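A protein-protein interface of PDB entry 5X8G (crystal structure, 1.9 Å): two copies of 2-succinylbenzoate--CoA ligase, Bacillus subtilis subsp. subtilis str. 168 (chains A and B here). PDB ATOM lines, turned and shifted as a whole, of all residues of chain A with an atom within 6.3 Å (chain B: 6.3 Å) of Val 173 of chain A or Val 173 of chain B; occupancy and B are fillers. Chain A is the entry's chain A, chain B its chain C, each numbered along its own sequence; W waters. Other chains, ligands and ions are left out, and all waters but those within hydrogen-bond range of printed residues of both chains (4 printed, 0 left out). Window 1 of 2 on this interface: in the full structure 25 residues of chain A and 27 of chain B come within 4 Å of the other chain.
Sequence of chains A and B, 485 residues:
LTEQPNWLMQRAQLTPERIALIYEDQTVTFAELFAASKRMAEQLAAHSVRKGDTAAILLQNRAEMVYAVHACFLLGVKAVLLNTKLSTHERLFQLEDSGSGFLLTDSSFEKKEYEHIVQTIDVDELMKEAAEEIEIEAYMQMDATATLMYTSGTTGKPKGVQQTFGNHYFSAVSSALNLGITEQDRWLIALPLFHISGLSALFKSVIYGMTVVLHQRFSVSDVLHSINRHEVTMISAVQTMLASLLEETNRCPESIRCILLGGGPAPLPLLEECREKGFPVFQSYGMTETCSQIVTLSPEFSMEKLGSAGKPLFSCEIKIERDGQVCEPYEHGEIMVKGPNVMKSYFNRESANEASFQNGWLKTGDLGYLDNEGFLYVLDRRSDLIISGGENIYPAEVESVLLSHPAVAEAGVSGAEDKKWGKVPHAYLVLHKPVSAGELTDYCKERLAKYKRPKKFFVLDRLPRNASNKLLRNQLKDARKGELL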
ATOM      1  N   HIS A 168      -8.551  33.367   6.082  1.00  0.00           N
ATOM      2  CA  HIS A 168      -9.320  32.955   7.253  1.00  0.00           C
ATOM      3  C   HIS A 168      -9.865  31.536   7.110  1.00  0.00           C
ATOM      4  O   HIS A 168      -9.921  30.790   8.094  1.00  0.00           O
ATOM      5  CB  HIS A 168     -10.471  33.937   7.502  1.00  0.00           C
ATOM      6  CG  HIS A 168     -10.020  35.334   7.797  1.00  0.00           C
ATOM      7  ND1 HIS A 168      -9.056  35.624   8.745  1.00  0.00           N
ATOM      8  CD2 HIS A 168     -10.417  36.527   7.286  1.00  0.00           C
ATOM      9  CE1 HIS A 168      -8.879  36.935   8.800  1.00  0.00           C
ATOM     10  NE2 HIS A 168      -9.688  37.507   7.920  1.00  0.00           N
ATOM     11  N   TYR A 169     -10.321  31.160   5.914  1.00  0.00           N
ATOM     12  CA  TYR A 169     -10.820  29.798   5.722  1.00  0.00           C
ATOM     13  C   TYR A 169      -9.719  28.783   6.016  1.00  0.00           C
ATOM     14  O   TYR A 169      -9.923  27.821   6.766  1.00  0.00           O
ATOM     15  CB  TYR A 169     -11.364  29.623   4.296  1.00  0.00           C
ATOM     16  CG  TYR A 169     -11.669  28.169   3.928  1.00  0.00           C
ATOM     17  CD1 TYR A 169     -12.916  27.606   4.193  1.00  0.00           C
ATOM     18  CD2 TYR A 169     -10.697  27.365   3.336  1.00  0.00           C
ATOM     19  CE1 TYR A 169     -13.190  26.258   3.857  1.00  0.00           C
ATOM     20  CE2 TYR A 169     -10.951  26.038   3.010  1.00  0.00           C
ATOM     21  CZ  TYR A 169     -12.186  25.489   3.283  1.00  0.00           C
ATOM     22  OH  TYR A 169     -12.411  24.169   2.954  1.00  0.00           O
ATOM     23  N   PHE A 170      -8.533  28.999   5.455  1.00  0.00           N
ATOM     24  CA  PHE A 170      -7.471  27.998   5.611  1.00  0.00           C
ATOM     25  C   PHE A 170      -6.902  28.001   7.020  1.00  0.00           C
ATOM     26  O   PHE A 170      -6.522  26.940   7.534  1.00  0.00           O
ATOM     27  CB  PHE A 170      -6.366  28.236   4.579  1.00  0.00           C
ATOM     28  CG  PHE A 170      -6.674  27.655   3.234  1.00  0.00           C
ATOM     29  CD1 PHE A 170      -6.590  26.283   3.028  1.00  0.00           C
ATOM     30  CD2 PHE A 170      -7.060  28.465   2.184  1.00  0.00           C
ATOM     31  CE1 PHE A 170      -6.880  25.730   1.790  1.00  0.00           C
ATOM     32  CE2 PHE A 170      -7.356  27.922   0.938  1.00  0.00           C
ATOM     33  CZ  PHE A 170      -7.262  26.546   0.745  1.00  0.00           C
ATOM     34  N   SER A 171      -6.837  29.169   7.670  1.00  0.00           N
ATOM     35  CA  SER A 171      -6.459  29.192   9.084  1.00  0.00           C
ATOM     36  C   SER A 171      -7.397  28.313   9.906  1.00  0.00           C
ATOM     37  O   SER A 171      -6.958  27.503  10.727  1.00  0.00           O
ATOM     38  CB  SER A 171      -6.488  30.632   9.613  1.00  0.00           C
ATOM     39  OG  SER A 171      -6.274  30.639  11.018  1.00  0.00           O
ATOM     40  N   ALA A 172      -8.706  28.452   9.675  1.00  0.00           N
ATOM     41  CA  ALA A 172      -9.688  27.681  10.441  1.00  0.00           C
ATOM     42  C   ALA A 172      -9.593  26.186  10.134  1.00  0.00           C
ATOM     43  O   ALA A 172      -9.732  25.348  11.039  1.00  0.00           O
ATOM     44  CB  ALA A 172     -11.101  28.199  10.129  1.00  0.00           C
ATOM     45  N   VAL A 173      -9.381  25.830   8.868  1.00  0.00           N
ATOM     46  CA  VAL A 173      -9.326  24.414   8.498  1.00  0.00           C
ATOM     47  C   VAL A 173      -8.059  23.767   9.052  1.00  0.00           C
ATOM     48  O   VAL A 173      -8.111  22.693   9.663  1.00  0.00           O
ATOM     49  CB  VAL A 173      -9.431  24.241   6.972  1.00  0.00           C
ATOM     50  CG1 VAL A 173      -9.030  22.824   6.560  1.00  0.00           C
ATOM     51  CG2 VAL A 173     -10.890  24.522   6.507  1.00  0.00           C
ATOM     52  N   SER A 174      -6.908  24.415   8.856  1.00  0.00           N
ATOM     53  CA  SER A 174      -5.645  23.865   9.358  1.00  0.00           C
ATOM     54  C   SER A 174      -5.676  23.698  10.874  1.00  0.00           C
ATOM     55  O   SER A 174      -5.101  22.745  11.413  1.00  0.00           O
ATOM     56  CB  SER A 174      -4.470  24.757   8.947  1.00  0.00           C
ATOM     57  OG  SER A 174      -4.255  24.714   7.538  1.00  0.00           O
ATOM     58  N   SER A 175      -6.314  24.630  11.586  1.00  0.00           N
ATOM     59  CA  SER A 175      -6.420  24.467  13.036  1.00  0.00           C
ATOM     60  C   SER A 175      -7.318  23.295  13.397  1.00  0.00           C
ATOM     61  O   SER A 175      -7.013  22.542  14.329  1.00  0.00           O
ATOM     62  CB  SER A 175      -6.947  25.741  13.698  1.00  0.00           C
ATOM     63  OG  SER A 175      -7.019  25.544  15.105  1.00  0.00           O
ATOM     64  N   ALA A 176      -8.448  23.138  12.689  1.00  0.00           N
ATOM     65  CA  ALA A 176      -9.312  21.981  12.920  1.00  0.00           C
ATOM     66  C   ALA A 176      -8.572  20.672  12.660  1.00  0.00           C
ATOM     67  O   ALA A 176      -8.757  19.688  13.386  1.00  0.00           O
ATOM     68  CB  ALA A 176     -10.559  22.065  12.023  1.00  0.00           C
ATOM     69  N   LEU A 177      -7.749  20.625  11.612  1.00  0.00           N
ATOM     70  CA  LEU A 177      -7.009  19.393  11.342  1.00  0.00           C
ATOM     71  C   LEU A 177      -6.002  19.098  12.449  1.00  0.00           C
ATOM     72  O   LEU A 177      -5.698  17.928  12.728  1.00  0.00           O
ATOM     73  CB  LEU A 177      -6.299  19.498   9.996  1.00  0.00           C
ATOM     74  CG  LEU A 177      -7.190  19.523   8.746  1.00  0.00           C
ATOM     75  CD1 LEU A 177      -6.340  19.851   7.534  1.00  0.00           C
ATOM     76  CD2 LEU A 177      -7.854  18.181   8.570  1.00  0.00           C
ATOM     77  N   ASN A 178      -5.485  20.143  13.087  1.00  0.00           N
ATOM     78  CA  ASN A 178      -4.507  19.966  14.154  1.00  0.00           C
ATOM     79  C   ASN A 178      -5.184  19.560  15.457  1.00  0.00           C
ATOM     80  O   ASN A 178      -4.745  18.623  16.129  1.00  0.00           O
ATOM     81  CB  ASN A 178      -3.709  21.262  14.336  1.00  0.00           C
ATOM     82  CG  ASN A 178      -2.705  21.166  15.463  1.00  0.00           C
ATOM     83  OD1 ASN A 178      -2.729  21.947  16.409  1.00  0.00           O
ATOM     84  ND2 ASN A 178      -1.833  20.192  15.373  1.00  0.00           N
ATOM     85  N   ILE A 207     -17.645  28.375  10.098  1.00  0.00           N
ATOM     86  CA  ILE A 207     -17.181  27.265   9.259  1.00  0.00           C
ATOM     87  C   ILE A 207     -17.419  25.922   9.950  1.00  0.00           C
ATOM     88  O   ILE A 207     -17.903  24.968   9.327  1.00  0.00           O
ATOM     89  CB  ILE A 207     -15.711  27.479   8.869  1.00  0.00           C
ATOM     90  CG1 ILE A 207     -15.586  28.688   7.941  1.00  0.00           C
ATOM     91  CG2 ILE A 207     -15.117  26.224   8.203  1.00  0.00           C
ATOM     92  CD1 ILE A 207     -14.128  29.200   7.790  1.00  0.00           C
ATOM     93  N   TYR A 208     -17.104  25.825  11.248  1.00  0.00           N
ATOM     94  CA  TYR A 208     -17.315  24.579  11.987  1.00  0.00           C
ATOM     95  C   TYR A 208     -18.775  24.364  12.362  1.00  0.00           C
ATOM     96  O   TYR A 208     -19.197  23.220  12.536  1.00  0.00           O
ATOM     97  CB  TYR A 208     -16.534  24.568  13.298  1.00  0.00           C
ATOM     98  CG  TYR A 208     -15.045  24.818  13.231  1.00  0.00           C
ATOM     99  CD1 TYR A 208     -14.346  24.872  12.012  1.00  0.00           C
ATOM    100  CD2 TYR A 208     -14.328  24.960  14.419  1.00  0.00           C
ATOM    101  CE1 TYR A 208     -12.954  25.115  11.992  1.00  0.00           C
ATOM    102  CE2 TYR A 208     -12.955  25.201  14.416  1.00  0.00           C
ATOM    103  CZ  TYR A 208     -12.271  25.274  13.207  1.00  0.00           C
ATOM    104  OH  TYR A 208     -10.902  25.515  13.269  1.00  0.00           O
ATOM    105  N   HIS B 168      -9.675  16.776  -4.282  1.00  0.00           N
ATOM    106  CA  HIS B 168      -9.556  15.789  -3.219  1.00  0.00           C
ATOM    107  C   HIS B 168      -9.371  16.451  -1.856  1.00  0.00           C
ATOM    108  O   HIS B 168      -9.924  15.980  -0.855  1.00  0.00           O
ATOM    109  CB  HIS B 168      -8.377  14.844  -3.510  1.00  0.00           C
ATOM    110  CG  HIS B 168      -8.569  13.989  -4.726  1.00  0.00           C
ATOM    111  ND1 HIS B 168      -9.716  13.251  -4.948  1.00  0.00           N
ATOM    112  CD2 HIS B 168      -7.740  13.716  -5.765  1.00  0.00           C
ATOM    113  CE1 HIS B 168      -9.590  12.576  -6.080  1.00  0.00           C
ATOM    114  NE2 HIS B 168      -8.397  12.836  -6.590  1.00  0.00           N
ATOM    115  N   TYR B 169      -8.556  17.505  -1.787  1.00  0.00           N
ATOM    116  CA  TYR B 169      -8.394  18.237  -0.531  1.00  0.00           C
ATOM    117  C   TYR B 169      -9.735  18.784  -0.048  1.00  0.00           C
ATOM    118  O   TYR B 169     -10.110  18.625   1.120  1.00  0.00           O
ATOM    119  CB  TYR B 169      -7.384  19.382  -0.706  1.00  0.00           C
ATOM    120  CG  TYR B 169      -7.332  20.337   0.470  1.00  0.00           C
ATOM    121  CD1 TYR B 169      -6.501  20.082   1.565  1.00  0.00           C
ATOM    122  CD2 TYR B 169      -8.117  21.499   0.494  1.00  0.00           C
ATOM    123  CE1 TYR B 169      -6.448  20.955   2.642  1.00  0.00           C
ATOM    124  CE2 TYR B 169      -8.076  22.370   1.570  1.00  0.00           C
ATOM    125  CZ  TYR B 169      -7.243  22.090   2.647  1.00  0.00           C
ATOM    126  OH  TYR B 169      -7.202  22.961   3.720  1.00  0.00           O
ATOM    127  N   PHE B 170     -10.491  19.414  -0.936  1.00  0.00           N
ATOM    128  CA  PHE B 170     -11.722  20.041  -0.459  1.00  0.00           C
ATOM    129  C   PHE B 170     -12.772  19.001  -0.095  1.00  0.00           C
ATOM    130  O   PHE B 170     -13.512  19.185   0.874  1.00  0.00           O
ATOM    131  CB  PHE B 170     -12.238  21.045  -1.480  1.00  0.00           C
ATOM    132  CG  PHE B 170     -11.564  22.381  -1.369  1.00  0.00           C
ATOM    133  CD1 PHE B 170     -11.866  23.228  -0.316  1.00  0.00           C
ATOM    134  CD2 PHE B 170     -10.603  22.772  -2.286  1.00  0.00           C
ATOM    135  CE1 PHE B 170     -11.239  24.455  -0.193  1.00  0.00           C
ATOM    136  CE2 PHE B 170      -9.967  24.000  -2.169  1.00  0.00           C
ATOM    137  CZ  PHE B 170     -10.287  24.837  -1.119  1.00  0.00           C
ATOM    138  N   SER B 171     -12.833  17.889  -0.835  1.00  0.00           N
ATOM    139  CA  SER B 171     -13.714  16.794  -0.431  1.00  0.00           C
ATOM    140  C   SER B 171     -13.404  16.337   0.997  1.00  0.00           C
ATOM    141  O   SER B 171     -14.313  16.175   1.823  1.00  0.00           O
ATOM    142  CB  SER B 171     -13.582  15.623  -1.415  1.00  0.00           C
ATOM    143  OG  SER B 171     -14.351  14.514  -0.986  1.00  0.00           O
ATOM    144  N   ALA B 172     -12.118  16.117   1.307  1.00  0.00           N
ATOM    145  CA  ALA B 172     -11.766  15.605   2.631  1.00  0.00           C
ATOM    146  C   ALA B 172     -12.073  16.627   3.721  1.00  0.00           C
ATOM    147  O   ALA B 172     -12.607  16.279   4.789  1.00  0.00           O
ATOM    148  CB  ALA B 172     -10.275  15.207   2.660  1.00  0.00           C
ATOM    149  N   VAL B 173     -11.758  17.894   3.463  1.00  0.00           N
ATOM    150  CA  VAL B 173     -12.042  18.955   4.428  1.00  0.00           C
ATOM    151  C   VAL B 173     -13.549  19.109   4.657  1.00  0.00           C
ATOM    152  O   VAL B 173     -14.016  19.155   5.803  1.00  0.00           O
ATOM    153  CB  VAL B 173     -11.397  20.272   3.966  1.00  0.00           C
ATOM    154  CG1 VAL B 173     -11.946  21.435   4.787  1.00  0.00           C
ATOM    155  CG2 VAL B 173      -9.876  20.177   4.120  1.00  0.00           C
ATOM    156  N   SER B 174     -14.334  19.196   3.580  1.00  0.00           N
ATOM    157  CA  SER B 174     -15.778  19.372   3.758  1.00  0.00           C
ATOM    158  C   SER B 174     -16.401  18.199   4.506  1.00  0.00           C
ATOM    159  O   SER B 174     -17.294  18.395   5.335  1.00  0.00           O
ATOM    160  CB  SER B 174     -16.468  19.568   2.406  1.00  0.00           C
ATOM    161  OG  SER B 174     -16.088  20.799   1.820  1.00  0.00           O
ATOM    162  N   SER B 175     -15.930  16.969   4.246  1.00  0.00           N
ATOM    163  CA  SER B 175     -16.451  15.818   4.986  1.00  0.00           C
ATOM    164  C   SER B 175     -16.086  15.889   6.469  1.00  0.00           C
ATOM    165  O   SER B 175     -16.908  15.551   7.333  1.00  0.00           O
ATOM    166  CB  SER B 175     -15.938  14.510   4.372  1.00  0.00           C
ATOM    167  OG  SER B 175     -16.425  13.384   5.100  1.00  0.00           O
ATOM    168  N   ALA B 176     -14.859  16.299   6.787  1.00  0.00           N
ATOM    169  CA  ALA B 176     -14.463  16.449   8.191  1.00  0.00           C
ATOM    170  C   ALA B 176     -15.311  17.509   8.892  1.00  0.00           C
ATOM    171  O   ALA B 176     -15.682  17.352  10.064  1.00  0.00           O
ATOM    172  CB  ALA B 176     -12.983  16.829   8.283  1.00  0.00           C
ATOM    173  N   LEU B 177     -15.606  18.605   8.203  1.00  0.00           N
ATOM    174  CA  LEU B 177     -16.467  19.616   8.817  1.00  0.00           C
ATOM    175  C   LEU B 177     -17.854  19.060   9.104  1.00  0.00           C
ATOM    176  O   LEU B 177     -18.509  19.493  10.063  1.00  0.00           O
ATOM    177  CB  LEU B 177     -16.559  20.852   7.925  1.00  0.00           C
ATOM    178  CG  LEU B 177     -15.276  21.665   7.725  1.00  0.00           C
ATOM    179  CD1 LEU B 177     -15.498  22.788   6.727  1.00  0.00           C
ATOM    180  CD2 LEU B 177     -14.762  22.232   9.038  1.00  0.00           C
ATOM    181  N   ASN B 178     -18.316  18.095   8.298  1.00  0.00           N
ATOM    182  CA  ASN B 178     -19.648  17.525   8.484  1.00  0.00           C
ATOM    183  C   ASN B 178     -19.661  16.491   9.601  1.00  0.00           C
ATOM    184  O   ASN B 178     -20.550  16.508  10.461  1.00  0.00           O
ATOM    185  CB  ASN B 178     -20.146  16.892   7.175  1.00  0.00           C
ATOM    186  CG  ASN B 178     -21.547  16.275   7.306  1.00  0.00           C
ATOM    187  OD1 ASN B 178     -21.756  15.097   6.998  1.00  0.00           O
ATOM    188  ND2 ASN B 178     -22.504  17.070   7.756  1.00  0.00           N
ATOM    189  N   ILE B 207      -4.438  13.695   4.993  1.00  0.00           N
ATOM    190  CA  ILE B 207      -4.796  15.053   5.395  1.00  0.00           C
ATOM    191  C   ILE B 207      -5.169  15.103   6.874  1.00  0.00           C
ATOM    192  O   ILE B 207      -4.743  16.010   7.598  1.00  0.00           O
ATOM    193  CB  ILE B 207      -5.916  15.609   4.495  1.00  0.00           C
ATOM    194  CG1 ILE B 207      -5.381  15.817   3.069  1.00  0.00           C
ATOM    195  CG2 ILE B 207      -6.427  16.939   5.049  1.00  0.00           C
ATOM    196  CD1 ILE B 207      -6.527  16.038   1.995  1.00  0.00           C
ATOM    197  N   TYR B 208      -5.947  14.128   7.357  1.00  0.00           N
ATOM    198  CA  TYR B 208      -6.313  14.118   8.773  1.00  0.00           C
ATOM    199  C   TYR B 208      -5.218  13.543   9.655  1.00  0.00           C
ATOM    200  O   TYR B 208      -5.202  13.826  10.854  1.00  0.00           O
ATOM    201  CB  TYR B 208      -7.562  13.273   9.055  1.00  0.00           C
ATOM    202  CG  TYR B 208      -8.801  13.515   8.213  1.00  0.00           C
ATOM    203  CD1 TYR B 208      -8.962  14.669   7.448  1.00  0.00           C
ATOM    204  CD2 TYR B 208      -9.832  12.578   8.217  1.00  0.00           C
ATOM    205  CE1 TYR B 208     -10.129  14.869   6.668  1.00  0.00           C
ATOM    206  CE2 TYR B 208     -10.991  12.770   7.457  1.00  0.00           C
ATOM    207  CZ  TYR B 208     -11.138  13.905   6.686  1.00  0.00           C
ATOM    208  OH  TYR B 208     -12.312  14.075   5.940  1.00  0.00           O
HETATM  209  O   HOH W   1      -5.310  22.879   5.624  1.00  0.00           O
HETATM  210  O   HOH W   2     -17.374  20.839  11.940  1.00  0.00           O
HETATM  211  O   HOH W   3      -7.108  15.757  11.734  1.00  0.00           O
HETATM  212  O   HOH W   4     -14.896  23.148   2.904  1.00  0.00           O
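Among the printed residues, merely in contact across the chains: Tyr 169 of chain A with Val 173 of chain B (3.3 Å), Tyr 169 of chain A with Phe 170 of chain B (3.4 Å), Val 173 of chain A with Tyr 169 of chain B (3.4 Å), Phe 170 of chain A with Tyr 169 of chain B (3.4 Å), Val 173 of chain A with Val 173 of chain B (3.7 Å), Ile 207 of chain A with Leu 177 of chain B (3.8 Å), Leu 177 of chain A with Ile 207 of chain B (3.8 Å), Leu 177 of chain A with Tyr 208 of chain B (3.8 Å), Phe 170 of chain A with Phe 170 of chain B (3.9 Å) and Tyr 208 of chain A with Leu 177 of chain B (3.998 Å).
Of the printed residues of chain B, Tyr 169 of chain A touches Phe 170 and Val 173.
Ala 176 of chain A touches none of the printed residues of chain B.
Printed residues of chain A within 4 Å of Phe 170 of chain B: Tyr 169 and Phe 170.
Printed residues of chain A within 4 Å of Val 173 of chain B: Tyr 169 (3.3 Å) and Val 173 (3.7 Å).
The nearest residue of chain B that does not touch Val 173 of chain A is Leu 177 of chain B (4.9 Å).
The nearest residue of chain A that does not touch Val 173 of chain B is Leu 177 of chain A (4.9 Å).
Hydrophobic or aromatic side chains of chain B that line the printed part of chain A: Tyr 169, Phe 170, Val 173, Leu 177, Ile 207 and Tyr 208.
Printed residues of chain A that touch a printed residue of chain B: Tyr 169, Phe 170, Val 173, Leu 177, Ile 207 and Tyr 208.
Hydrophobic or aromatic side chains of chain A within 4 Å of the printed part of chain B: Tyr 169, Phe 170, Val 173, Leu 177, Ile 207 and Tyr 208.
Among the printed residues, 10 pairs touch across the chains.
Tyr 169 of chain A touches Phe 170 of chain B, and with the chains exchanged Phe 170 of chain A touches Tyr 169 of chain B.
Phe 170 of chain A touches its own counterpart, Phe 170 of chain B.
Val 173 of chain B touches its own counterpart, Val 173 of chain A.
Leu 177 of chain A touches Tyr 208 of chain B, and with the chains exchanged Tyr 208 of chain A touches Leu 177 of chain B.
Water W2 lies within hydrogen-bond range of the backbone carbonyl oxygen (O) of Leu 177 of chain B (2.6 Å) and the backbone carbonyl oxygen (O) of Tyr 208 of chain A (3.1 Å).
Water W1 bridges the side-chain hydroxyl of Tyr 169 of chain B and the side-chain hydroxyl of Ser 174 of chain A.
Water W4 bridges OH of Tyr 169 of chain A (2.7 Å) and OG of Ser 174 of chain B (2.8 Å).
Water W3 lies within hydrogen-bond range of O of Leu 177 of chain A (2.8 Å) and O of Tyr 208 of chain B (2.9 Å).
The side-chain hydroxyl (OH) of Tyr 208 of chain A sits at hydrogen-bond distance from the backbone carbonyl oxygen (O) of Ala 172 of chain A, at 2.5 Å.
The backbone NH of Ala 176 of chain B is in hydrogen-bond range of the side-chain hydroxyl of Tyr 208 of chain B (3.5 Å).
O of Phe 170 of chain A sits at hydrogen-bond distance from OG of Ser 174 of chain A (3.2 Å).
OG of Ser 174 of chain B lies within hydrogen-bond range of O of Phe 170 of chain B.
The backbone NH (N) of Ala 176 of chain A sits at hydrogen-bond distance from the side-chain hydroxyl (OH) of Tyr 208 of chain A (3.5 Å).
The side-chain hydroxyl of Tyr 208 of chain B is in hydrogen-bond range of the backbone carbonyl oxygen of Ala 172 of chain B, 2.5 Å away.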
